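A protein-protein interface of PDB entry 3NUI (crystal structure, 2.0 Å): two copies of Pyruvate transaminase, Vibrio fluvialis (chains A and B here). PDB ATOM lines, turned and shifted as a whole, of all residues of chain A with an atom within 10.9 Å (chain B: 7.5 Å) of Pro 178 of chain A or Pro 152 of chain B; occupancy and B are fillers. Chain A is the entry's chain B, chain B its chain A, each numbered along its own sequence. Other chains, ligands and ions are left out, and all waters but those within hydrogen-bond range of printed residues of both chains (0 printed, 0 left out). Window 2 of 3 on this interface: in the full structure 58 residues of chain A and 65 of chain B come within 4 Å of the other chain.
The backbone carbonyl oxygen of Arg 155 of chain B is in hydrogen-bond range of the indole nitrogen of Trp 143 of chain B (2.8 Å).
Among the printed residues, merely in contact across the chains: Pro 178 of chain A with Pro 152 of chain B (3.7 Å), Tyr 179 of chain A with Phe 144 of chain B (3.6 Å), Tyr 179 of chain A with Ala 147 of chain B (3.9 Å), Tyr 179 of chain A with Ala 148 of chain B (3.98 Å), Val 182 of chain A with Trp 143 of chain B (3.8 Å), Val 182 of chain A with Phe 144 of chain B (3.9 Å) and Phe 183 of chain A with Phe 144 of chain B (3.6 Å).
Met 174 of chain A touches none of the printed residues of chain B.
Of chain B, only Pro 152 comes within 4 Å of Pro 178 of chain A.
Asn 180 of chain A touches none of the printed residues of chain B.
Printed residues of chain A within 4 Å of Trp 143 of chain B: Val 182.
Of the printed residues of chain A, Ala 148 of chain B touches Tyr 179 (3.98 Å).
No residue of chain A comes within 4 Å of Gly 150 of chain B.
Of chain A, only Pro 178 comes within 4 Å of Pro 152 of chain B.
No residue of chain A comes within 4 Å of Gln 153 of chain B.
The nearest residue of chain A that does not touch Pro 152 of chain B is Tyr 179 of chain A (6.2 Å).
Of the 16 printed residues of chain A, 4 touch a printed residue of chain B.
Printed residues of chain A that touch a printed residue of chain B: Pro 178, Tyr 179, Val 182 and Phe 183.
Hydrophobic or aromatic side chains of chain A within 4 Å of the printed part of chain B: Pro 178, Tyr 179, Val 182 and Phe 183.
Hydrophobic or aromatic side chains of chain B that line the printed part of chain A: Trp 143, Phe 144, Ala 147 and Pro 152.
Among the printed residues, 7 pairs touch across the chains.
No position is printed for both chains.
Of the 7 pairs that touch across the chains among the printed residues, none has its exchanged pair printed and touching as well.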
ATOM      1  N   TRP A 161      32.307  29.099  14.768  1.00  0.00           N
ATOM      2  CA  TRP A 161      31.614  27.774  14.572  1.00  0.00           C
ATOM      3  C   TRP A 161      30.354  27.855  13.664  1.00  0.00           C
ATOM      4  O   TRP A 161      29.589  28.836  13.763  1.00  0.00           O
ATOM      5  CB  TRP A 161      31.187  27.156  15.909  1.00  0.00           C
ATOM      6  CG  TRP A 161      30.497  25.808  15.720  1.00  0.00           C
ATOM      7  CD1 TRP A 161      31.096  24.576  15.684  1.00  0.00           C
ATOM      8  CD2 TRP A 161      29.080  25.577  15.476  1.00  0.00           C
ATOM      9  NE1 TRP A 161      30.149  23.596  15.446  1.00  0.00           N
ATOM     10  CE2 TRP A 161      28.907  24.182  15.316  1.00  0.00           C
ATOM     11  CE3 TRP A 161      27.949  26.419  15.388  1.00  0.00           C
ATOM     12  CZ2 TRP A 161      27.632  23.594  15.072  1.00  0.00           C
ATOM     13  CZ3 TRP A 161      26.685  25.842  15.127  1.00  0.00           C
ATOM     14  CH2 TRP A 161      26.546  24.439  14.966  1.00  0.00           C
ATOM     15  N   ALA A 163      27.302  24.833  11.442  1.00  0.00           N
ATOM     16  CA  ALA A 163      26.988  23.438  11.016  1.00  0.00           C
ATOM     17  C   ALA A 163      27.342  23.181   9.532  1.00  0.00           C
ATOM     18  O   ALA A 163      27.391  24.130   8.755  1.00  0.00           O
ATOM     19  CB  ALA A 163      25.526  23.115  11.298  1.00  0.00           C
ATOM     20  N   TYR A 164      27.606  21.918   9.153  1.00  0.00           N
ATOM     21  CA  TYR A 164      27.769  21.516   7.715  1.00  0.00           C
ATOM     22  C   TYR A 164      26.421  21.417   7.013  1.00  0.00           C
ATOM     23  O   TYR A 164      25.517  20.771   7.549  1.00  0.00           O
ATOM     24  CB  TYR A 164      28.514  20.163   7.537  1.00  0.00           C
ATOM     25  CG  TYR A 164      30.001  20.228   7.833  1.00  0.00           C
ATOM     26  CD1 TYR A 164      30.871  20.956   6.990  1.00  0.00           C
ATOM     27  CD2 TYR A 164      30.547  19.570   8.960  1.00  0.00           C
ATOM     28  CE1 TYR A 164      32.256  21.036   7.257  1.00  0.00           C
ATOM     29  CE2 TYR A 164      31.935  19.637   9.242  1.00  0.00           C
ATOM     30  CZ  TYR A 164      32.780  20.376   8.378  1.00  0.00           C
ATOM     31  OH  TYR A 164      34.136  20.453   8.626  1.00  0.00           O
ATOM     32  N   MET A 174      13.336  22.487   2.358  1.00  0.00           N
ATOM     33  CA  MET A 174      13.404  22.145   3.800  1.00  0.00           C
ATOM     34  C   MET A 174      14.093  23.192   4.716  1.00  0.00           C
ATOM     35  O   MET A 174      14.972  23.949   4.288  1.00  0.00           O
ATOM     36  CB  MET A 174      14.005  20.718   3.995  1.00  0.00           C
ATOM     37  CG  MET A 174      12.989  19.562   4.311  1.00  0.00           C
ATOM     38  SD  MET A 174      11.380  19.525   3.424  1.00  0.00           S
ATOM     39  CE  MET A 174      10.445  18.280   4.347  1.00  0.00           C
ATOM     40  N   THR A 175      13.670  23.200   5.980  1.00  0.00           N
ATOM     41  CA  THR A 175      14.073  24.195   6.977  1.00  0.00           C
ATOM     42  C   THR A 175      15.407  23.817   7.636  1.00  0.00           C
ATOM     43  O   THR A 175      16.147  24.679   8.152  1.00  0.00           O
ATOM     44  CB  THR A 175      12.937  24.406   8.052  1.00  0.00           C
ATOM     45  OG1 THR A 175      13.108  23.509   9.160  1.00  0.00           O
ATOM     46  CG2 THR A 175      11.514  24.217   7.437  1.00  0.00           C
ATOM     47  N   GLY A 176      15.713  22.519   7.593  1.00  0.00           N
ATOM     48  CA  GLY A 176      16.892  21.969   8.243  1.00  0.00           C
ATOM     49  C   GLY A 176      16.508  20.973   9.328  1.00  0.00           C
ATOM     50  O   GLY A 176      15.333  20.824   9.689  1.00  0.00           O
ATOM     51  N   LYS A 177      17.509  20.284   9.857  1.00  0.00           N
ATOM     52  CA  LYS A 177      17.255  19.236  10.836  1.00  0.00           C
ATOM     53  C   LYS A 177      17.979  19.558  12.137  1.00  0.00           C
ATOM     54  O   LYS A 177      19.205  19.753  12.134  1.00  0.00           O
ATOM     55  CB  LYS A 177      17.648  17.858  10.292  1.00  0.00           C
ATOM     56  CG  LYS A 177      18.538  17.856   9.042  1.00  0.00           C
ATOM     57  CD  LYS A 177      17.721  17.478   7.802  1.00  0.00           C
ATOM     58  CE  LYS A 177      18.526  16.568   6.871  1.00  0.00           C
ATOM     59  NZ  LYS A 177      17.634  15.650   6.109  1.00  0.00           N
ATOM     60  N   PRO A 178      17.218  19.618  13.253  1.00  0.00           N
ATOM     61  CA  PRO A 178      17.760  20.060  14.554  1.00  0.00           C
ATOM     62  C   PRO A 178      18.848  19.116  15.112  1.00  0.00           C
ATOM     63  O   PRO A 178      19.794  19.585  15.771  1.00  0.00           O
ATOM     64  CB  PRO A 178      16.517  20.120  15.460  1.00  0.00           C
ATOM     65  CG  PRO A 178      15.529  19.180  14.826  1.00  0.00           C
ATOM     66  CD  PRO A 178      15.796  19.223  13.342  1.00  0.00           C
ATOM     67  N   TYR A 179      18.735  17.816  14.798  1.00  0.00           N
ATOM     68  CA  TYR A 179      19.693  16.786  15.252  1.00  0.00           C
ATOM     69  C   TYR A 179      21.090  16.878  14.613  1.00  0.00           C
ATOM     70  O   TYR A 179      22.051  16.354  15.182  1.00  0.00           O
ATOM     71  CB  TYR A 179      19.132  15.374  15.016  1.00  0.00           C
ATOM     72  CG  TYR A 179      18.816  15.132  13.569  1.00  0.00           C
ATOM     73  CD1 TYR A 179      17.513  15.306  13.092  1.00  0.00           C
ATOM     74  CD2 TYR A 179      19.826  14.786  12.657  1.00  0.00           C
ATOM     75  CE1 TYR A 179      17.206  15.110  11.746  1.00  0.00           C
ATOM     76  CE2 TYR A 179      19.540  14.602  11.290  1.00  0.00           C
ATOM     77  CZ  TYR A 179      18.220  14.760  10.844  1.00  0.00           C
ATOM     78  OH  TYR A 179      17.910  14.571   9.513  1.00  0.00           O
ATOM     79  N   ASN A 180      21.200  17.516  13.442  1.00  0.00           N
ATOM     80  CA  ASN A 180      22.499  17.629  12.737  1.00  0.00           C
ATOM     81  C   ASN A 180      23.525  18.597  13.392  1.00  0.00           C
ATOM     82  O   ASN A 180      24.713  18.495  13.128  1.00  0.00           O
ATOM     83  CB  ASN A 180      22.338  17.780  11.180  1.00  0.00           C
ATOM     84  CG  ASN A 180      22.651  19.207  10.644  1.00  0.00           C
ATOM     85  OD1 ASN A 180      22.271  20.228  11.231  1.00  0.00           O
ATOM     86  ND2 ASN A 180      23.340  19.261   9.503  1.00  0.00           N
ATOM     87  N   SER A 181      23.075  19.492  14.273  1.00  0.00           N
ATOM     88  CA  SER A 181      24.011  20.343  15.003  1.00  0.00           C
ATOM     89  C   SER A 181      23.835  20.282  16.537  1.00  0.00           C
ATOM     90  O   SER A 181      23.730  21.321  17.186  1.00  0.00           O
ATOM     91  CB  SER A 181      23.890  21.795  14.530  1.00  0.00           C
ATOM     92  OG  SER A 181      22.757  22.411  15.126  1.00  0.00           O
ATOM     93  N   VAL A 182      23.791  19.082  17.110  1.00  0.00           N
ATOM     94  CA  VAL A 182      23.632  18.922  18.574  1.00  0.00           C
ATOM     95  C   VAL A 182      25.031  18.754  19.132  1.00  0.00           C
ATOM     96  O   VAL A 182      25.401  19.398  20.107  1.00  0.00           O
ATOM     97  CB  VAL A 182      22.705  17.686  18.969  1.00  0.00           C
ATOM     98  CG1 VAL A 182      22.903  17.233  20.452  1.00  0.00           C
ATOM     99  CG2 VAL A 182      21.225  17.970  18.632  1.00  0.00           C
ATOM    100  N   PHE A 183      25.812  17.898  18.478  1.00  0.00           N
ATOM    101  CA  PHE A 183      27.090  17.488  19.059  1.00  0.00           C
ATOM    102  C   PHE A 183      28.208  18.521  18.969  1.00  0.00           C
ATOM    103  O   PHE A 183      29.065  18.582  19.850  1.00  0.00           O
ATOM    104  CB  PHE A 183      27.524  16.128  18.536  1.00  0.00           C
ATOM    105  CG  PHE A 183      26.800  15.001  19.164  1.00  0.00           C
ATOM    106  CD1 PHE A 183      27.164  14.545  20.453  1.00  0.00           C
ATOM    107  CD2 PHE A 183      25.750  14.387  18.496  1.00  0.00           C
ATOM    108  CE1 PHE A 183      26.485  13.491  21.050  1.00  0.00           C
ATOM    109  CE2 PHE A 183      25.086  13.312  19.085  1.00  0.00           C
ATOM    110  CZ  PHE A 183      25.457  12.862  20.356  1.00  0.00           C
ATOM    111  N   GLY A 184      28.205  19.316  17.913  1.00  0.00           N
ATOM    112  CA  GLY A 184      29.120  20.437  17.864  1.00  0.00           C
ATOM    113  C   GLY A 184      28.644  21.695  18.589  1.00  0.00           C
ATOM    114  O   GLY A 184      29.477  22.525  18.947  1.00  0.00           O
ATOM    115  N   LEU A 185      27.325  21.848  18.812  1.00  0.00           N
ATOM    116  CA  LEU A 185      26.779  23.149  19.269  1.00  0.00           C
ATOM    117  C   LEU A 185      27.598  23.782  20.408  1.00  0.00           C
ATOM    118  O   LEU A 185      27.854  23.148  21.431  1.00  0.00           O
ATOM    119  CB  LEU A 185      25.267  23.087  19.592  1.00  0.00           C
ATOM    120  CG  LEU A 185      24.493  24.433  19.775  1.00  0.00           C
ATOM    121  CD1 LEU A 185      24.207  25.200  18.432  1.00  0.00           C
ATOM    122  CD2 LEU A 185      23.204  24.287  20.618  1.00  0.00           C
ATOM    123  N   PRO A 186      28.042  25.044  20.227  1.00  0.00           N
ATOM    124  CA  PRO A 186      28.734  25.632  21.363  1.00  0.00           C
ATOM    125  C   PRO A 186      27.740  25.887  22.496  1.00  0.00           C
ATOM    126  O   PRO A 186      26.503  25.702  22.318  1.00  0.00           O
ATOM    127  CB  PRO A 186      29.303  26.960  20.803  1.00  0.00           C
ATOM    128  CG  PRO A 186      29.127  26.839  19.249  1.00  0.00           C
ATOM    129  CD  PRO A 186      27.937  25.979  19.086  1.00  0.00           C
ATOM    130  N   TRP B 143      19.431  14.541  23.401  1.00  0.00           N
ATOM    131  CA  TRP B 143      18.957  15.660  22.558  1.00  0.00           C
ATOM    132  C   TRP B 143      18.912  15.173  21.117  1.00  0.00           C
ATOM    133  O   TRP B 143      17.886  15.308  20.398  1.00  0.00           O
ATOM    134  CB  TRP B 143      19.868  16.859  22.695  1.00  0.00           C
ATOM    135  CG  TRP B 143      19.791  17.538  23.997  1.00  0.00           C
ATOM    136  CD1 TRP B 143      18.780  17.414  24.943  1.00  0.00           C
ATOM    137  CD2 TRP B 143      20.742  18.452  24.537  1.00  0.00           C
ATOM    138  NE1 TRP B 143      19.046  18.224  26.018  1.00  0.00           N
ATOM    139  CE2 TRP B 143      20.236  18.887  25.791  1.00  0.00           C
ATOM    140  CE3 TRP B 143      21.963  18.999  24.058  1.00  0.00           C
ATOM    141  CZ2 TRP B 143      20.924  19.815  26.612  1.00  0.00           C
ATOM    142  CZ3 TRP B 143      22.630  19.929  24.850  1.00  0.00           C
ATOM    143  CH2 TRP B 143      22.114  20.331  26.130  1.00  0.00           C
ATOM    144  N   PHE B 144      20.016  14.557  20.705  1.00  0.00           N
ATOM    145  CA  PHE B 144      20.104  14.057  19.381  1.00  0.00           C
ATOM    146  C   PHE B 144      18.979  13.078  19.070  1.00  0.00           C
ATOM    147  O   PHE B 144      18.274  13.238  18.059  1.00  0.00           O
ATOM    148  CB  PHE B 144      21.446  13.395  19.142  1.00  0.00           C
ATOM    149  CG  PHE B 144      21.455  12.544  17.902  1.00  0.00           C
ATOM    150  CD1 PHE B 144      21.716  13.124  16.661  1.00  0.00           C
ATOM    151  CD2 PHE B 144      21.230  11.184  17.964  1.00  0.00           C
ATOM    152  CE1 PHE B 144      21.724  12.343  15.496  1.00  0.00           C
ATOM    153  CE2 PHE B 144      21.235  10.397  16.777  1.00  0.00           C
ATOM    154  CZ  PHE B 144      21.477  10.997  15.572  1.00  0.00           C
ATOM    155  N   LEU B 145      18.775  12.097  19.959  1.00  0.00           N
ATOM    156  CA  LEU B 145      17.762  11.101  19.763  1.00  0.00           C
ATOM    157  C   LEU B 145      16.351  11.674  19.638  1.00  0.00           C
ATOM    158  O   LEU B 145      15.581  11.356  18.637  1.00  0.00           O
ATOM    159  CB  LEU B 145      17.779  10.105  20.930  1.00  0.00           C
ATOM    160  CG  LEU B 145      16.771   9.006  20.703  1.00  0.00           C
ATOM    161  CD1 LEU B 145      17.128   8.201  19.349  1.00  0.00           C
ATOM    162  CD2 LEU B 145      16.722   8.104  21.927  1.00  0.00           C
ATOM    163  N   HIS B 146      15.976  12.491  20.631  1.00  0.00           N
ATOM    164  CA  HIS B 146      14.621  13.020  20.640  1.00  0.00           C
ATOM    165  C   HIS B 146      14.383  13.914  19.397  1.00  0.00           C
ATOM    166  O   HIS B 146      13.282  13.912  18.856  1.00  0.00           O
ATOM    167  CB  HIS B 146      14.315  13.823  21.897  1.00  0.00           C
ATOM    168  CG  HIS B 146      14.435  13.033  23.169  1.00  0.00           C
ATOM    169  ND1 HIS B 146      13.770  11.843  23.386  1.00  0.00           N
ATOM    170  CD2 HIS B 146      15.134  13.288  24.303  1.00  0.00           C
ATOM    171  CE1 HIS B 146      14.055  11.395  24.602  1.00  0.00           C
ATOM    172  NE2 HIS B 146      14.896  12.242  25.170  1.00  0.00           N
ATOM    173  N   ALA B 147      15.389  14.675  18.987  1.00  0.00           N
ATOM    174  CA  ALA B 147      15.283  15.498  17.792  1.00  0.00           C
ATOM    175  C   ALA B 147      15.054  14.643  16.533  1.00  0.00           C
ATOM    176  O   ALA B 147      14.223  14.995  15.672  1.00  0.00           O
ATOM    177  CB  ALA B 147      16.486  16.340  17.652  1.00  0.00           C
ATOM    178  N   ALA B 148      15.751  13.515  16.442  1.00  0.00           N
ATOM    179  CA  ALA B 148      15.620  12.598  15.315  1.00  0.00           C
ATOM    180  C   ALA B 148      14.287  11.917  15.341  1.00  0.00           C
ATOM    181  O   ALA B 148      13.779  11.509  14.287  1.00  0.00           O
ATOM    182  CB  ALA B 148      16.749  11.591  15.291  1.00  0.00           C
ATOM    183  N   GLU B 149      13.700  11.801  16.537  1.00  0.00           N
ATOM    184  CA  GLU B 149      12.337  11.284  16.714  1.00  0.00           C
ATOM    185  C   GLU B 149      11.203  12.330  16.600  1.00  0.00           C
ATOM    186  O   GLU B 149      10.078  12.075  17.015  1.00  0.00           O
ATOM    187  CB  GLU B 149      12.229  10.528  18.039  1.00  0.00           C
ATOM    188  CG  GLU B 149      13.077   9.286  18.045  1.00  0.00           C
ATOM    189  CD  GLU B 149      12.890   8.458  19.313  1.00  0.00           C
ATOM    190  OE1 GLU B 149      12.241   8.965  20.251  1.00  0.00           O
ATOM    191  OE2 GLU B 149      13.386   7.305  19.363  1.00  0.00           O
ATOM    192  N   GLY B 150      11.514  13.504  16.085  1.00  0.00           N
ATOM    193  CA  GLY B 150      10.502  14.543  15.870  1.00  0.00           C
ATOM    194  C   GLY B 150      10.085  15.256  17.141  1.00  0.00           C
ATOM    195  O   GLY B 150       9.009  15.854  17.196  1.00  0.00           O
ATOM    196  N   LYS B 151      10.909  15.194  18.188  1.00  0.00           N
ATOM    197  CA  LYS B 151      10.629  15.989  19.376  1.00  0.00           C
ATOM    198  C   LYS B 151      11.819  16.836  19.827  1.00  0.00           C
ATOM    199  O   LYS B 151      12.424  16.571  20.868  1.00  0.00           O
ATOM    200  CB  LYS B 151      10.098  15.084  20.497  1.00  0.00           C
ATOM    201  CG  LYS B 151       8.668  14.611  20.175  1.00  0.00           C
ATOM    202  CD  LYS B 151       8.109  13.460  21.042  1.00  0.00           C
ATOM    203  CE  LYS B 151       7.388  12.494  20.082  1.00  0.00           C
ATOM    204  NZ  LYS B 151       6.778  11.398  20.818  1.00  0.00           N
ATOM    205  N   PRO B 152      12.169  17.867  19.033  1.00  0.00           N
ATOM    206  CA  PRO B 152      13.426  18.522  19.328  1.00  0.00           C
ATOM    207  C   PRO B 152      13.240  19.446  20.507  1.00  0.00           C
ATOM    208  O   PRO B 152      14.190  20.062  20.927  1.00  0.00           O
ATOM    209  CB  PRO B 152      13.701  19.348  18.047  1.00  0.00           C
ATOM    210  CG  PRO B 152      12.342  19.548  17.445  1.00  0.00           C
ATOM    211  CD  PRO B 152      11.619  18.285  17.721  1.00  0.00           C
ATOM    212  N   GLN B 153      12.020  19.557  21.033  1.00  0.00           N
ATOM    213  CA  GLN B 153      11.845  20.376  22.239  1.00  0.00           C
ATOM    214  C   GLN B 153      12.126  19.526  23.487  1.00  0.00           C
ATOM    215  O   GLN B 153      12.066  20.018  24.595  1.00  0.00           O
ATOM    216  CB  GLN B 153      10.422  20.966  22.302  1.00  0.00           C
ATOM    217  CG  GLN B 153       9.310  19.970  22.587  1.00  0.00           C
ATOM    218  CD  GLN B 153       8.801  19.186  21.373  1.00  0.00           C
ATOM    219  OE1 GLN B 153       9.502  18.952  20.383  1.00  0.00           O
ATOM    220  NE2 GLN B 153       7.561  18.764  21.459  1.00  0.00           N
ATOM    221  N   LYS B 154      12.408  18.250  23.301  1.00  0.00           N
ATOM    222  CA  LYS B 154      12.510  17.330  24.460  1.00  0.00           C
ATOM    223  C   LYS B 154      13.957  17.502  24.896  1.00  0.00           C
ATOM    224  O   LYS B 154      14.869  16.836  24.382  1.00  0.00           O
ATOM    225  CB  LYS B 154      12.158  15.899  24.051  1.00  0.00           C
ATOM    226  CG  LYS B 154      11.754  15.009  25.243  1.00  0.00           C
ATOM    227  CD  LYS B 154      11.266  13.623  24.758  1.00  0.00           C
ATOM    228  CE  LYS B 154      11.194  12.584  25.906  1.00  0.00           C
ATOM    229  NZ  LYS B 154      10.100  12.888  26.857  1.00  0.00           N
ATOM    230  N   ARG B 155      14.169  18.486  25.763  1.00  0.00           N
ATOM    231  CA  ARG B 155      15.516  18.892  26.123  1.00  0.00           C
ATOM    232  C   ARG B 155      15.851  18.984  27.579  1.00  0.00           C
ATOM    233  O   ARG B 155      17.068  18.970  27.929  1.00  0.00           O
ATOM    234  CB  ARG B 155      15.821  20.237  25.453  1.00  0.00           C
ATOM    235  CG  ARG B 155      16.094  20.008  23.921  1.00  0.00           C
ATOM    236  CD  ARG B 155      16.459  21.304  23.200  1.00  0.00           C
ATOM    237  NE  ARG B 155      17.705  21.880  23.690  1.00  0.00           N
ATOM    238  CZ  ARG B 155      18.912  21.575  23.197  1.00  0.00           C
ATOM    239  NH1 ARG B 155      20.003  22.170  23.654  1.00  0.00           N
ATOM    240  NH2 ARG B 155      19.026  20.708  22.222  1.00  0.00           N
ATOM    241  N   ASP B 229       6.716  16.158  27.081  1.00  0.00           N
ATOM    242  CA  ASP B 229       7.337  16.390  25.765  1.00  0.00           C
ATOM    243  C   ASP B 229       8.578  17.291  25.770  1.00  0.00           C
ATOM    244  O   ASP B 229       9.309  17.296  24.793  1.00  0.00           O
ATOM    245  CB  ASP B 229       6.294  16.962  24.758  1.00  0.00           C
ATOM    246  CG  ASP B 229       5.992  18.435  25.028  1.00  0.00           C
ATOM    247  OD1 ASP B 229       6.073  19.270  24.066  1.00  0.00           O
ATOM    248  OD2 ASP B 229       5.683  18.783  26.211  1.00  0.00           O
ATOM    249  N   THR B 230       8.807  18.080  26.820  1.00  0.00           N
ATOM    250  CA  THR B 230       9.956  18.953  26.842  1.00  0.00           C
ATOM    251  C   THR B 230      11.110  18.397  27.697  1.00  0.00           C
ATOM    252  O   THR B 230      12.094  19.064  27.863  1.00  0.00           O
ATOM    253  CB  THR B 230       9.637  20.371  27.356  1.00  0.00           C
ATOM    254  OG1 THR B 230       9.427  20.303  28.763  1.00  0.00           O
ATOM    255  CG2 THR B 230       8.366  21.054  26.639  1.00  0.00           C
